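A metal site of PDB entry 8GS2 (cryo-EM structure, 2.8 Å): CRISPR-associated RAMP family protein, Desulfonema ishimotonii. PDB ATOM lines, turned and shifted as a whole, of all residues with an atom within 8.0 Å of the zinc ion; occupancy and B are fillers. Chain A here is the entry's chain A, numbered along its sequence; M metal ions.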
ATOM      1  N   ARG A 452      30.599  24.449  -6.643  1.00  0.00           N
ATOM      2  CA  ARG A 452      30.596  25.606  -7.546  1.00  0.00           C
ATOM      3  C   ARG A 452      31.280  26.802  -6.898  1.00  0.00           C
ATOM      4  O   ARG A 452      32.048  27.521  -7.548  1.00  0.00           O
ATOM      5  CB  ARG A 452      29.163  25.947  -7.943  1.00  0.00           C
ATOM      6  CG  ARG A 452      29.042  27.129  -8.888  1.00  0.00           C
ATOM      7  CD  ARG A 452      27.592  27.414  -9.227  1.00  0.00           C
ATOM      8  NE  ARG A 452      26.990  26.323  -9.976  1.00  0.00           N
ATOM      9  CZ  ARG A 452      27.003  26.218 -11.295  1.00  0.00           C
ATOM     10  NH1 ARG A 452      27.611  27.118 -12.051  1.00  0.00           N
ATOM     11  NH2 ARG A 452      26.404  25.185 -11.873  1.00  0.00           N
ATOM     12  N   GLN A 456      34.658  28.601  -8.345  1.00  0.00           N
ATOM     13  CA  GLN A 456      34.744  30.033  -8.602  1.00  0.00           C
ATOM     14  C   GLN A 456      35.845  30.692  -7.782  1.00  0.00           C
ATOM     15  O   GLN A 456      36.503  31.625  -8.263  1.00  0.00           O
ATOM     16  CB  GLN A 456      33.400  30.707  -8.324  1.00  0.00           C
ATOM     17  CG  GLN A 456      32.294  30.297  -9.281  1.00  0.00           C
ATOM     18  CD  GLN A 456      30.985  30.969  -8.949  1.00  0.00           C
ATOM     19  OE1 GLN A 456      30.654  32.019  -9.506  1.00  0.00           O
ATOM     20  NE2 GLN A 456      30.221  30.367  -8.055  1.00  0.00           N
ATOM     21  N   SER A 461      37.008  34.155 -10.421  1.00  0.00           N
ATOM     22  CA  SER A 461      36.137  34.822 -11.390  1.00  0.00           C
ATOM     23  C   SER A 461      34.703  34.415 -11.128  1.00  0.00           C
ATOM     24  O   SER A 461      34.308  33.292 -11.487  1.00  0.00           O
ATOM     25  CB  SER A 461      36.541  34.486 -12.818  1.00  0.00           C
ATOM     26  OG  SER A 461      36.448  33.099 -13.062  1.00  0.00           O
ATOM     27  N   PRO A 462      33.889  35.272 -10.508  1.00  0.00           N
ATOM     28  CA  PRO A 462      32.486  34.920 -10.257  1.00  0.00           C
ATOM     29  C   PRO A 462      31.732  34.728 -11.563  1.00  0.00           C
ATOM     30  O   PRO A 462      32.012  35.366 -12.573  1.00  0.00           O
ATOM     31  CB  PRO A 462      31.943  36.121  -9.471  1.00  0.00           C
ATOM     32  CG  PRO A 462      33.163  36.789  -8.914  1.00  0.00           C
ATOM     33  CD  PRO A 462      34.237  36.575  -9.922  1.00  0.00           C
ATOM     34  N   CYS A 463      30.748  33.837 -11.522  1.00  0.00           N
ATOM     35  CA  CYS A 463      29.879  33.579 -12.670  1.00  0.00           C
ATOM     36  C   CYS A 463      28.653  34.468 -12.547  1.00  0.00           C
ATOM     37  O   CYS A 463      27.725  34.176 -11.776  1.00  0.00           O
ATOM     38  CB  CYS A 463      29.498  32.103 -12.741  1.00  0.00           C
ATOM     39  SG  CYS A 463      28.340  31.727 -14.073  1.00  0.00           S
ATOM     40  N   ASN A 464      28.643  35.572 -13.292  1.00  0.00           N
ATOM     41  CA  ASN A 464      27.526  36.511 -13.262  1.00  0.00           C
ATOM     42  C   ASN A 464      26.485  36.151 -14.326  1.00  0.00           C
ATOM     43  O   ASN A 464      26.192  36.915 -15.241  1.00  0.00           O
ATOM     44  CB  ASN A 464      28.043  37.938 -13.448  1.00  0.00           C
ATOM     45  CG  ASN A 464      28.960  38.380 -12.322  1.00  0.00           C
ATOM     46  OD1 ASN A 464      28.759  38.019 -11.162  1.00  0.00           O
ATOM     47  ND2 ASN A 464      29.977  39.152 -12.659  1.00  0.00           N
ATOM     48  N   ALA A 465      25.940  34.952 -14.172  1.00  0.00           N
ATOM     49  CA  ALA A 465      24.919  34.438 -15.071  1.00  0.00           C
ATOM     50  C   ALA A 465      23.555  34.462 -14.393  1.00  0.00           C
ATOM     51  O   ALA A 465      23.451  34.585 -13.170  1.00  0.00           O
ATOM     52  CB  ALA A 465      25.253  33.010 -15.515  1.00  0.00           C
ATOM     53  N   GLU A 466      22.520  34.354 -15.217  1.00  0.00           N
ATOM     54  CA  GLU A 466      21.145  34.373 -14.743  1.00  0.00           C
ATOM     55  C   GLU A 466      20.416  33.130 -15.236  1.00  0.00           C
ATOM     56  O   GLU A 466      20.752  32.563 -16.276  1.00  0.00           O
ATOM     57  CB  GLU A 466      20.415  35.640 -15.223  1.00  0.00           C
ATOM     58  CG  GLU A 466      19.013  35.836 -14.665  1.00  0.00           C
ATOM     59  CD  GLU A 466      19.001  35.993 -13.154  1.00  0.00           C
ATOM     60  OE1 GLU A 466      20.019  36.473 -12.591  1.00  0.00           O
ATOM     61  OE2 GLU A 466      17.987  35.638 -12.526  1.00  0.00           O
ATOM     62  N   PRO A 471      23.038  27.627 -22.216  1.00  0.00           N
ATOM     63  CA  PRO A 471      23.939  27.316 -21.106  1.00  0.00           C
ATOM     64  C   PRO A 471      25.143  28.253 -21.055  1.00  0.00           C
ATOM     65  O   PRO A 471      25.680  28.657 -22.076  1.00  0.00           O
ATOM     66  CB  PRO A 471      24.374  25.876 -21.409  1.00  0.00           C
ATOM     67  CG  PRO A 471      23.266  25.320 -22.220  1.00  0.00           C
ATOM     68  CD  PRO A 471      22.770  26.455 -23.059  1.00  0.00           C
ATOM     69  N   CYS A 472      25.544  28.594 -19.835  1.00  0.00           N
ATOM     70  CA  CYS A 472      26.712  29.428 -19.636  1.00  0.00           C
ATOM     71  C   CYS A 472      27.978  28.696 -20.055  1.00  0.00           C
ATOM     72  O   CYS A 472      28.131  27.492 -19.800  1.00  0.00           O
ATOM     73  CB  CYS A 472      26.822  29.861 -18.174  1.00  0.00           C
ATOM     74  SG  CYS A 472      28.220  30.932 -17.801  1.00  0.00           S
ATOM     75  N   MET A 473      28.885  29.408 -20.703  1.00  0.00           N
ATOM     76  CA  MET A 473      30.106  28.820 -21.250  1.00  0.00           C
ATOM     77  C   MET A 473      31.340  29.141 -20.417  1.00  0.00           C
ATOM     78  O   MET A 473      32.467  28.929 -20.876  1.00  0.00           O
ATOM     79  CB  MET A 473      30.307  29.278 -22.696  1.00  0.00           C
ATOM     80  CG  MET A 473      29.173  28.889 -23.623  1.00  0.00           C
ATOM     81  SD  MET A 473      28.826  27.126 -23.605  1.00  0.00           S
ATOM     82  CE  MET A 473      30.428  26.463 -24.050  1.00  0.00           C
ATOM     83  N   CYS A 474      31.156  29.650 -19.200  1.00  0.00           N
ATOM     84  CA  CYS A 474      32.297  29.896 -18.338  1.00  0.00           C
ATOM     85  C   CYS A 474      32.878  28.563 -17.860  1.00  0.00           C
ATOM     86  O   CYS A 474      32.216  27.525 -17.860  1.00  0.00           O
ATOM     87  CB  CYS A 474      31.914  30.766 -17.148  1.00  0.00           C
ATOM     88  SG  CYS A 474      31.229  29.881 -15.736  1.00  0.00           S
ATOM     89  N   LYS A 475      34.146  28.610 -17.452  1.00  0.00           N
ATOM     90  CA  LYS A 475      34.858  27.385 -17.093  1.00  0.00           C
ATOM     91  C   LYS A 475      34.224  26.691 -15.895  1.00  0.00           C
ATOM     92  O   LYS A 475      34.156  25.453 -15.862  1.00  0.00           O
ATOM     93  CB  LYS A 475      36.332  27.692 -16.822  1.00  0.00           C
ATOM     94  CG  LYS A 475      36.589  29.137 -16.411  1.00  0.00           C
ATOM     95  CD  LYS A 475      38.060  29.485 -16.490  1.00  0.00           C
ATOM     96  CE  LYS A 475      38.310  30.930 -16.102  1.00  0.00           C
ATOM     97  NZ  LYS A 475      39.741  31.296 -16.144  1.00  0.00           N
ATOM     98  N   THR A 476      33.754  27.456 -14.904  1.00  0.00           N
ATOM     99  CA  THR A 476      33.097  26.850 -13.751  1.00  0.00           C
ATOM    100  C   THR A 476      31.838  26.102 -14.155  1.00  0.00           C
ATOM    101  O   THR A 476      31.613  24.964 -13.722  1.00  0.00           O
ATOM    102  CB  THR A 476      32.783  27.917 -12.707  1.00  0.00           C
ATOM    103  OG1 THR A 476      33.976  28.604 -12.333  1.00  0.00           O
ATOM    104  CG2 THR A 476      32.162  27.296 -11.477  1.00  0.00           C
ATOM    105  N   CYS A 477      31.007  26.727 -14.997  1.00  0.00           N
ATOM    106  CA  CYS A 477      29.790  26.058 -15.458  1.00  0.00           C
ATOM    107  C   CYS A 477      30.103  24.859 -16.348  1.00  0.00           C
ATOM    108  O   CYS A 477      29.405  23.840 -16.278  1.00  0.00           O
ATOM    109  CB  CYS A 477      28.894  27.041 -16.199  1.00  0.00           C
ATOM    110  SG  CYS A 477      27.950  28.150 -15.136  1.00  0.00           S
ATOM    111  N   ARG A 478      31.137  24.969 -17.188  1.00  0.00           N
ATOM    112  CA  ARG A 478      31.533  23.829 -18.011  1.00  0.00           C
ATOM    113  C   ARG A 478      31.966  22.651 -17.151  1.00  0.00           C
ATOM    114  O   ARG A 478      31.617  21.501 -17.447  1.00  0.00           O
ATOM    115  CB  ARG A 478      32.659  24.236 -18.966  1.00  0.00           C
ATOM    116  CG  ARG A 478      32.192  25.035 -20.167  1.00  0.00           C
ATOM    117  CD  ARG A 478      33.359  25.307 -21.104  1.00  0.00           C
ATOM    118  NE  ARG A 478      34.269  26.297 -20.547  1.00  0.00           N
ATOM    119  CZ  ARG A 478      35.526  26.458 -20.944  1.00  0.00           C
ATOM    120  NH1 ARG A 478      36.065  25.687 -21.870  1.00  0.00           N
ATOM    121  NH2 ARG A 478      36.266  27.421 -20.382  1.00  0.00           N
ATOM    122  N   MET A 480      30.985  22.140 -13.997  1.00  0.00           N
ATOM    123  CA  MET A 480      29.850  21.685 -13.205  1.00  0.00           C
ATOM    124  C   MET A 480      28.859  20.884 -14.048  1.00  0.00           C
ATOM    125  O   MET A 480      28.187  19.999 -13.506  1.00  0.00           O
ATOM    126  CB  MET A 480      29.138  22.870 -12.554  1.00  0.00           C
ATOM    127  CG  MET A 480      29.946  23.541 -11.454  1.00  0.00           C
ATOM    128  SD  MET A 480      30.375  22.419 -10.116  1.00  0.00           S
ATOM    129  CE  MET A 480      28.761  21.938  -9.533  1.00  0.00           C
ATOM    130  N   ARG A 481      28.751  21.168 -15.343  1.00  0.00           N
ATOM    131  CA  ARG A 481      27.830  20.409 -16.183  1.00  0.00           C
ATOM    132  C   ARG A 481      28.259  18.953 -16.357  1.00  0.00           C
ATOM    133  O   ARG A 481      27.438  18.137 -16.782  1.00  0.00           O
ATOM    134  CB  ARG A 481      27.681  21.075 -17.546  1.00  0.00           C
ATOM    135  CG  ARG A 481      26.772  22.291 -17.538  1.00  0.00           C
ATOM    136  CD  ARG A 481      26.278  22.637 -18.934  1.00  0.00           C
ATOM    137  NE  ARG A 481      27.366  23.003 -19.829  1.00  0.00           N
ATOM    138  CZ  ARG A 481      27.799  24.241 -20.026  1.00  0.00           C
ATOM    139  NH1 ARG A 481      27.253  25.264 -19.397  1.00  0.00           N
ATOM    140  NH2 ARG A 481      28.803  24.460 -20.875  1.00  0.00           N
HETATM  141 ZN    ZN M   1      28.919  30.179 -15.706  1.00  0.00          ZN
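NH1 of Arg 452 lies close to SG of Cys 477 (3.3 Å). N of Cys 463 lies within hydrogen-bond range of OE1 of Gln 456 (2.7 Å). SG of Cys 474 lies close to N of Thr 476 (3.6 Å). The guanidinium group (NH1) of Arg 481 lies within hydrogen-bond range of the backbone carbonyl oxygen (O) of Cys 472, 2.4 Å away.
The zinc ion is bound by SG of Cys 477 (2.3 Å), SG of Cys 463 (2.3 Å), SG of Cys 474 (2.3 Å) and SG of Cys 472 (2.3 Å). The zinc ion has four donor atoms within binding distance.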
